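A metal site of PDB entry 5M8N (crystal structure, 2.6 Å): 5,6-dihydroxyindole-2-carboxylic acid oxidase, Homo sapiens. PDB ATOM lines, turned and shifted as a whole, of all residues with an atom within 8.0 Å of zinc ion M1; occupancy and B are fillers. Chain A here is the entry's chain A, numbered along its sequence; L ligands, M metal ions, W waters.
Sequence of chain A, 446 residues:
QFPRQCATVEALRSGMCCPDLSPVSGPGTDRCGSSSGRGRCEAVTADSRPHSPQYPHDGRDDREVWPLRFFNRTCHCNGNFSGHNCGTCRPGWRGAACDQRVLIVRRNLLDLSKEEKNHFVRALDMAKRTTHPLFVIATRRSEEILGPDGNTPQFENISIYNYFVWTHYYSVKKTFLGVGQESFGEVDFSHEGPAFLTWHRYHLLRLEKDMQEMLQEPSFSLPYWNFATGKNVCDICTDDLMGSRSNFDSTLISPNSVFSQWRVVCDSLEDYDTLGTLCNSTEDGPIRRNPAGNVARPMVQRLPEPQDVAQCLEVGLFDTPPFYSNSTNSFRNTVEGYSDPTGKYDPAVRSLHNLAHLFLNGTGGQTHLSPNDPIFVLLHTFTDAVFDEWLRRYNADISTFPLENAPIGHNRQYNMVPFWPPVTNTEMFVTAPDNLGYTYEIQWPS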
ATOM      1  N   HIS A 168      20.771  17.384  17.772  1.00  0.00           N
ATOM      2  CA  HIS A 168      21.229  18.448  16.894  1.00  0.00           C
ATOM      3  C   HIS A 168      20.886  19.818  17.492  1.00  0.00           C
ATOM      4  O   HIS A 168      21.710  20.738  17.439  1.00  0.00           O
ATOM      5  CB  HIS A 168      20.593  18.270  15.515  1.00  0.00           C
ATOM      6  CG  HIS A 168      21.136  19.172  14.461  1.00  0.00           C
ATOM      7  ND1 HIS A 168      20.492  20.334  14.093  1.00  0.00           N
ATOM      8  CD2 HIS A 168      22.240  19.083  13.688  1.00  0.00           C
ATOM      9  CE1 HIS A 168      21.181  20.918  13.121  1.00  0.00           C
ATOM     10  NE2 HIS A 168      22.251  20.182  12.869  1.00  0.00           N
ATOM     11  N   TYR A 169      19.696  19.929  18.097  1.00  0.00           N
ATOM     12  CA  TYR A 169      19.299  21.154  18.777  1.00  0.00           C
ATOM     13  C   TYR A 169      20.200  21.412  19.980  1.00  0.00           C
ATOM     14  O   TYR A 169      20.706  22.518  20.190  1.00  0.00           O
ATOM     15  CB  TYR A 169      17.805  21.071  19.206  1.00  0.00           C
ATOM     16  CG  TYR A 169      17.505  21.822  20.497  1.00  0.00           C
ATOM     17  CD1 TYR A 169      17.189  23.181  20.472  1.00  0.00           C
ATOM     18  CD2 TYR A 169      17.577  21.195  21.744  1.00  0.00           C
ATOM     19  CE1 TYR A 169      16.943  23.885  21.664  1.00  0.00           C
ATOM     20  CE2 TYR A 169      17.350  21.898  22.942  1.00  0.00           C
ATOM     21  CZ  TYR A 169      17.026  23.237  22.877  1.00  0.00           C
ATOM     22  OH  TYR A 169      16.777  23.942  24.022  1.00  0.00           O
ATOM     23  N   SER A 171      23.200  20.314  20.587  1.00  0.00           N
ATOM     24  CA  SER A 171      24.522  20.758  20.155  1.00  0.00           C
ATOM     25  C   SER A 171      24.575  22.219  19.736  1.00  0.00           C
ATOM     26  O   SER A 171      25.688  22.741  19.595  1.00  0.00           O
ATOM     27  CB  SER A 171      24.997  19.908  18.976  1.00  0.00           C
ATOM     28  OG  SER A 171      24.130  20.065  17.859  1.00  0.00           O
ATOM     29  N   VAL A 172      23.448  22.900  19.494  1.00  0.00           N
ATOM     30  CA  VAL A 172      23.479  24.223  18.874  1.00  0.00           C
ATOM     31  C   VAL A 172      22.862  25.301  19.739  1.00  0.00           C
ATOM     32  O   VAL A 172      23.028  26.482  19.414  1.00  0.00           O
ATOM     33  CB  VAL A 172      22.815  24.253  17.473  1.00  0.00           C
ATOM     34  CG1 VAL A 172      23.414  23.199  16.548  1.00  0.00           C
ATOM     35  CG2 VAL A 172      21.245  24.187  17.564  1.00  0.00           C
ATOM     36  N   ASP A 188      28.726  26.895  18.891  1.00  0.00           N
ATOM     37  CA  ASP A 188      28.086  25.911  18.004  1.00  0.00           C
ATOM     38  C   ASP A 188      28.906  24.632  18.100  1.00  0.00           C
ATOM     39  O   ASP A 188      30.007  24.562  17.544  1.00  0.00           O
ATOM     40  CB  ASP A 188      28.007  26.427  16.576  1.00  0.00           C
ATOM     41  CG  ASP A 188      26.881  25.730  15.766  1.00  0.00           C
ATOM     42  OD1 ASP A 188      26.797  24.473  15.852  1.00  0.00           O
ATOM     43  OD2 ASP A 188      26.098  26.451  15.069  1.00  0.00           O
ATOM     44  N   SER A 190      28.403  21.761  16.767  1.00  0.00           N
ATOM     45  CA  SER A 190      28.303  20.885  15.602  1.00  0.00           C
ATOM     46  C   SER A 190      28.468  21.586  14.253  1.00  0.00           C
ATOM     47  O   SER A 190      28.424  20.904  13.210  1.00  0.00           O
ATOM     48  CB  SER A 190      26.968  20.134  15.628  1.00  0.00           C
ATOM     49  OG  SER A 190      25.922  20.980  16.068  1.00  0.00           O
ATOM     50  N   HIS A 191      28.645  22.906  14.246  1.00  0.00           N
ATOM     51  CA  HIS A 191      28.834  23.668  13.018  1.00  0.00           C
ATOM     52  C   HIS A 191      29.932  24.692  13.230  1.00  0.00           C
ATOM     53  O   HIS A 191      30.392  24.915  14.346  1.00  0.00           O
ATOM     54  CB  HIS A 191      27.530  24.372  12.596  1.00  0.00           C
ATOM     55  CG  HIS A 191      26.357  23.474  12.527  1.00  0.00           C
ATOM     56  ND1 HIS A 191      25.561  23.201  13.625  1.00  0.00           N
ATOM     57  CD2 HIS A 191      25.881  22.712  11.506  1.00  0.00           C
ATOM     58  CE1 HIS A 191      24.625  22.336  13.274  1.00  0.00           C
ATOM     59  NE2 HIS A 191      24.794  22.022  12.001  1.00  0.00           N
ATOM     60  N   PHE A 196      32.230  19.731  12.616  1.00  0.00           N
ATOM     61  CA  PHE A 196      31.072  19.612  11.730  1.00  0.00           C
ATOM     62  C   PHE A 196      30.927  18.232  11.063  1.00  0.00           C
ATOM     63  O   PHE A 196      29.931  17.530  11.252  1.00  0.00           O
ATOM     64  CB  PHE A 196      31.160  20.735  10.683  1.00  0.00           C
ATOM     65  CG  PHE A 196      30.129  20.643   9.609  1.00  0.00           C
ATOM     66  CD1 PHE A 196      28.801  20.775   9.898  1.00  0.00           C
ATOM     67  CD2 PHE A 196      30.496  20.427   8.286  1.00  0.00           C
ATOM     68  CE1 PHE A 196      27.831  20.692   8.892  1.00  0.00           C
ATOM     69  CE2 PHE A 196      29.558  20.341   7.277  1.00  0.00           C
ATOM     70  CZ  PHE A 196      28.216  20.474   7.576  1.00  0.00           C
ATOM     71  N   TRP A 199      30.794  15.284  13.519  1.00  0.00           N
ATOM     72  CA  TRP A 199      29.587  15.338  14.331  1.00  0.00           C
ATOM     73  C   TRP A 199      28.402  14.802  13.541  1.00  0.00           C
ATOM     74  O   TRP A 199      27.633  13.944  14.005  1.00  0.00           O
ATOM     75  CB  TRP A 199      29.352  16.800  14.801  1.00  0.00           C
ATOM     76  CG  TRP A 199      28.294  16.904  15.885  1.00  0.00           C
ATOM     77  CD1 TRP A 199      28.514  17.016  17.216  1.00  0.00           C
ATOM     78  CD2 TRP A 199      26.862  16.800  15.711  1.00  0.00           C
ATOM     79  NE1 TRP A 199      27.312  17.022  17.887  1.00  0.00           N
ATOM     80  CE2 TRP A 199      26.286  16.878  16.990  1.00  0.00           C
ATOM     81  CE3 TRP A 199      26.014  16.658  14.593  1.00  0.00           C
ATOM     82  CZ2 TRP A 199      24.895  16.803  17.200  1.00  0.00           C
ATOM     83  CZ3 TRP A 199      24.624  16.584  14.804  1.00  0.00           C
ATOM     84  CH2 TRP A 199      24.087  16.651  16.089  1.00  0.00           C
ATOM     85  N   HIS A 200      28.235  15.287  12.315  1.00  0.00           N
ATOM     86  CA  HIS A 200      27.099  14.832  11.526  1.00  0.00           C
ATOM     87  C   HIS A 200      27.274  13.389  11.078  1.00  0.00           C
ATOM     88  O   HIS A 200      26.270  12.691  10.917  1.00  0.00           O
ATOM     89  CB  HIS A 200      26.888  15.775  10.350  1.00  0.00           C
ATOM     90  CG  HIS A 200      26.370  17.118  10.779  1.00  0.00           C
ATOM     91  ND1 HIS A 200      27.148  18.042  11.455  1.00  0.00           N
ATOM     92  CD2 HIS A 200      25.126  17.665  10.706  1.00  0.00           C
ATOM     93  CE1 HIS A 200      26.428  19.112  11.731  1.00  0.00           C
ATOM     94  NE2 HIS A 200      25.193  18.903  11.293  1.00  0.00           N
ATOM     95  N   HIS A 203      26.087  11.486  14.042  1.00  0.00           N
ATOM     96  CA  HIS A 203      24.638  11.737  14.051  1.00  0.00           C
ATOM     97  C   HIS A 203      23.899  10.769  13.118  1.00  0.00           C
ATOM     98  O   HIS A 203      22.911  10.128  13.527  1.00  0.00           O
ATOM     99  CB  HIS A 203      24.388  13.193  13.641  1.00  0.00           C
ATOM    100  CG  HIS A 203      23.014  13.698  13.966  1.00  0.00           C
ATOM    101  ND1 HIS A 203      22.368  14.636  13.179  1.00  0.00           N
ATOM    102  CD2 HIS A 203      22.157  13.403  14.967  1.00  0.00           C
ATOM    103  CE1 HIS A 203      21.173  14.891  13.689  1.00  0.00           C
ATOM    104  NE2 HIS A 203      21.029  14.162  14.775  1.00  0.00           N
ATOM    105  N   GLU A 336      31.029  22.428   4.196  1.00  0.00           N
ATOM    106  CA  GLU A 336      30.009  23.027   5.057  1.00  0.00           C
ATOM    107  C   GLU A 336      29.313  24.181   4.368  1.00  0.00           C
ATOM    108  O   GLU A 336      28.085  24.301   4.416  1.00  0.00           O
ATOM    109  CB  GLU A 336      30.589  23.493   6.394  1.00  0.00           C
ATOM    110  CG  GLU A 336      29.559  24.093   7.342  1.00  0.00           C
ATOM    111  CD  GLU A 336      30.047  24.189   8.811  1.00  0.00           C
ATOM    112  OE1 GLU A 336      31.243  23.900   9.071  1.00  0.00           O
ATOM    113  OE2 GLU A 336      29.261  24.585   9.718  1.00  0.00           O
ATOM    114  N   HIS A 353      26.867  22.431   1.432  1.00  0.00           N
ATOM    115  CA  HIS A 353      25.973  21.947   2.491  1.00  0.00           C
ATOM    116  C   HIS A 353      25.023  23.033   3.014  1.00  0.00           C
ATOM    117  O   HIS A 353      23.854  22.749   3.303  1.00  0.00           O
ATOM    118  CB  HIS A 353      26.765  21.377   3.656  1.00  0.00           C
ATOM    119  CG  HIS A 353      26.026  21.403   4.958  1.00  0.00           C
ATOM    120  ND1 HIS A 353      26.192  22.418   5.888  1.00  0.00           N
ATOM    121  CD2 HIS A 353      25.148  20.533   5.511  1.00  0.00           C
ATOM    122  CE1 HIS A 353      25.456  22.169   6.948  1.00  0.00           C
ATOM    123  NE2 HIS A 353      24.805  21.032   6.746  1.00  0.00           N
ATOM    124  N   ASN A 354      25.522  24.269   3.188  1.00  0.00           N
ATOM    125  CA  ASN A 354      24.679  25.332   3.736  1.00  0.00           C
ATOM    126  C   ASN A 354      23.683  25.839   2.700  1.00  0.00           C
ATOM    127  O   ASN A 354      22.553  26.175   3.051  1.00  0.00           O
ATOM    128  CB  ASN A 354      25.514  26.502   4.255  1.00  0.00           C
ATOM    129  CG  ASN A 354      26.141  26.234   5.616  1.00  0.00           C
ATOM    130  OD1 ASN A 354      25.656  25.414   6.419  1.00  0.00           O
ATOM    131  ND2 ASN A 354      27.239  26.938   5.903  1.00  0.00           N
ATOM    132  N   HIS A 357      20.768  23.663   2.510  1.00  0.00           N
ATOM    133  CA  HIS A 357      19.855  23.882   3.631  1.00  0.00           C
ATOM    134  C   HIS A 357      18.932  25.051   3.355  1.00  0.00           C
ATOM    135  O   HIS A 357      17.711  24.950   3.478  1.00  0.00           O
ATOM    136  CB  HIS A 357      20.633  24.128   4.932  1.00  0.00           C
ATOM    137  CG  HIS A 357      20.871  22.881   5.740  1.00  0.00           C
ATOM    138  ND1 HIS A 357      19.846  22.192   6.355  1.00  0.00           N
ATOM    139  CD2 HIS A 357      22.011  22.213   6.033  1.00  0.00           C
ATOM    140  CE1 HIS A 357      20.345  21.146   6.992  1.00  0.00           C
ATOM    141  NE2 HIS A 357      21.655  21.135   6.806  1.00  0.00           N
ATOM    142  N   GLN A 366      16.806  26.271   9.081  1.00  0.00           N
ATOM    143  CA  GLN A 366      17.104  26.838  10.394  1.00  0.00           C
ATOM    144  C   GLN A 366      17.870  25.833  11.242  1.00  0.00           C
ATOM    145  O   GLN A 366      17.449  24.674  11.366  1.00  0.00           O
ATOM    146  CB  GLN A 366      15.843  27.245  11.140  1.00  0.00           C
ATOM    147  CG  GLN A 366      14.805  27.924  10.342  1.00  0.00           C
ATOM    148  CD  GLN A 366      13.504  27.915  11.104  1.00  0.00           C
ATOM    149  OE1 GLN A 366      12.558  27.300  10.691  1.00  0.00           O
ATOM    150  NE2 GLN A 366      13.467  28.582  12.245  1.00  0.00           N
ATOM    151  N   THR A 367      18.979  26.228  11.803  1.00  0.00           N
ATOM    152  CA  THR A 367      19.884  25.299  12.413  1.00  0.00           C
ATOM    153  C   THR A 367      19.349  24.558  13.596  1.00  0.00           C
ATOM    154  O   THR A 367      19.571  23.390  13.718  1.00  0.00           O
ATOM    155  CB  THR A 367      21.182  25.986  12.789  1.00  0.00           C
ATOM    156  OG1 THR A 367      21.519  26.862  11.735  1.00  0.00           O
ATOM    157  CG2 THR A 367      22.282  25.003  12.976  1.00  0.00           C
ATOM    158  N   HIS A 368      18.623  25.219  14.460  1.00  0.00           N
ATOM    159  CA  HIS A 368      18.036  24.490  15.585  1.00  0.00           C
ATOM    160  C   HIS A 368      16.878  23.572  15.183  1.00  0.00           C
ATOM    161  O   HIS A 368      16.513  22.701  15.970  1.00  0.00           O
ATOM    162  CB  HIS A 368      17.511  25.459  16.637  1.00  0.00           C
ATOM    163  CG  HIS A 368      16.398  26.312  16.139  1.00  0.00           C
ATOM    164  ND1 HIS A 368      16.553  27.181  15.085  1.00  0.00           N
ATOM    165  CD2 HIS A 368      15.095  26.392  16.522  1.00  0.00           C
ATOM    166  CE1 HIS A 368      15.396  27.780  14.847  1.00  0.00           C
ATOM    167  NE2 HIS A 368      14.504  27.319  15.703  1.00  0.00           N
ATOM    168  N   SER A 370      16.453  22.125  11.744  1.00  0.00           N
ATOM    169  CA  SER A 370      16.492  21.524  10.414  1.00  0.00           C
ATOM    170  C   SER A 370      16.295  20.008  10.372  1.00  0.00           C
ATOM    171  O   SER A 370      15.717  19.545   9.376  1.00  0.00           O
ATOM    172  CB  SER A 370      17.783  21.923   9.707  1.00  0.00           C
ATOM    173  OG  SER A 370      18.891  21.487  10.458  1.00  0.00           O
ATOM    174  N   PRO A 371      16.737  19.191  11.330  1.00  0.00           N
ATOM    175  CA  PRO A 371      16.471  17.738  11.201  1.00  0.00           C
ATOM    176  C   PRO A 371      15.001  17.401  11.252  1.00  0.00           C
ATOM    177  O   PRO A 371      14.639  16.255  10.961  1.00  0.00           O
ATOM    178  CB  PRO A 371      17.241  17.126  12.389  1.00  0.00           C
ATOM    179  CG  PRO A 371      18.265  18.127  12.710  1.00  0.00           C
ATOM    180  CD  PRO A 371      17.568  19.454  12.522  1.00  0.00           C
ATOM    181  N   PHE A 376      16.889  16.348   5.683  1.00  0.00           N
ATOM    182  CA  PHE A 376      18.127  16.505   6.448  1.00  0.00           C
ATOM    183  C   PHE A 376      18.991  15.266   6.379  1.00  0.00           C
ATOM    184  O   PHE A 376      20.181  15.336   6.072  1.00  0.00           O
ATOM    185  CB  PHE A 376      17.782  16.825   7.905  1.00  0.00           C
ATOM    186  CG  PHE A 376      18.968  17.148   8.730  1.00  0.00           C
ATOM    187  CD1 PHE A 376      19.662  16.136   9.400  1.00  0.00           C
ATOM    188  CD2 PHE A 376      19.394  18.460   8.860  1.00  0.00           C
ATOM    189  CE1 PHE A 376      20.762  16.438  10.164  1.00  0.00           C
ATOM    190  CE2 PHE A 376      20.483  18.771   9.627  1.00  0.00           C
ATOM    191  CZ  PHE A 376      21.174  17.752  10.273  1.00  0.00           C
ATOM    192  N   HIS A 380      22.455  15.188   4.587  1.00  0.00           N
ATOM    193  CA  HIS A 380      23.677  14.941   5.331  1.00  0.00           C
ATOM    194  C   HIS A 380      24.365  13.634   5.003  1.00  0.00           C
ATOM    195  O   HIS A 380      25.580  13.548   5.228  1.00  0.00           O
ATOM    196  CB  HIS A 380      23.397  15.036   6.825  1.00  0.00           C
ATOM    197  CG  HIS A 380      23.544  16.424   7.318  1.00  0.00           C
ATOM    198  ND1 HIS A 380      24.775  17.005   7.505  1.00  0.00           N
ATOM    199  CD2 HIS A 380      22.631  17.404   7.517  1.00  0.00           C
ATOM    200  CE1 HIS A 380      24.610  18.264   7.855  1.00  0.00           C
ATOM    201  NE2 HIS A 380      23.319  18.530   7.877  1.00  0.00           N
HETATM  202  O1  LIG L   1      23.515  23.466   9.491  1.00  0.00           O
HETATM  203  C1  LIG L   1      23.937  29.630   7.354  1.00  0.00           C
HETATM  204  O2  LIG L   1      24.196  29.506   6.170  1.00  0.00           O
HETATM  205  O3  LIG L   1      24.077  30.720   7.941  1.00  0.00           O
HETATM  206  N1  LIG L   1      22.589  29.027   9.144  1.00  0.00           N
HETATM  207  C2  LIG L   1      23.414  28.445   8.120  1.00  0.00           C
HETATM  208  C3  LIG L   1      22.653  27.528   7.170  1.00  0.00           C
HETATM  209  N2  LIG L   1      22.155  26.391   7.877  1.00  0.00           N
HETATM  210  C4  LIG L   1      23.092  25.397   8.358  1.00  0.00           C
HETATM  211  C5  LIG L   1      20.726  26.192   8.136  1.00  0.00           C
HETATM  212  C6  LIG L   1      22.647  24.370   9.007  1.00  0.00           C
HETATM  213  C7  LIG L   1      20.291  25.143   8.782  1.00  0.00           C
HETATM  214  C8  LIG L   1      21.227  24.148   9.292  1.00  0.00           C
HETATM  215  O4  LIG L   1      20.892  23.205   9.897  1.00  0.00           O
HETATM  216 ZN    ZN M   1      23.720  20.338  11.547  1.00  0.00          ZN
HETATM  217 ZN    ZN M   2      23.308  20.531   7.952  1.00  0.00          ZN
HETATM  218  O   HOH W   1      22.879  21.166   9.823  1.00  0.00           O
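An oxygen (O1) of the ligand lies close to a ring nitrogen (NE2) of His 191, 3.2 Å away. The side-chain hydroxyl of Ser 370 is in hydrogen-bond range of an oxygen (O4) of the ligand (2.7 Å).
A ring nitrogen (ND1) of His 200 lies within hydrogen-bond range of the backbone carbonyl oxygen (O) of Phe 196. A ring nitrogen (ND1) of His 168 lies close to the backbone carbonyl oxygen of Thr 367, at 3.2 Å. The backbone carbonyl oxygen (O) of His 168 sits at hydrogen-bond distance from the side-chain hydroxyl (OG) of Ser 171. ND1 of His 191 sits at hydrogen-bond distance from OG of Ser 190 (3.3 Å). ND1 of His 191 lies within hydrogen-bond range of OD1 of Asp 188, 2.8 Å away.
Phe 376 touches zinc ion M1. Four residues have an atom within 4 Å of zinc ion M1: His 168, His 191, His 200 and Phe 376. The nearest printed residue that does not touch zinc ion M1 is His 380 (4.1 Å).
Zinc ion M1 is bound by NE2 of His 168, NE2 of His 191, NE2 of His 200 and water W1. Zinc ion M1 has four donor atoms within binding distance.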
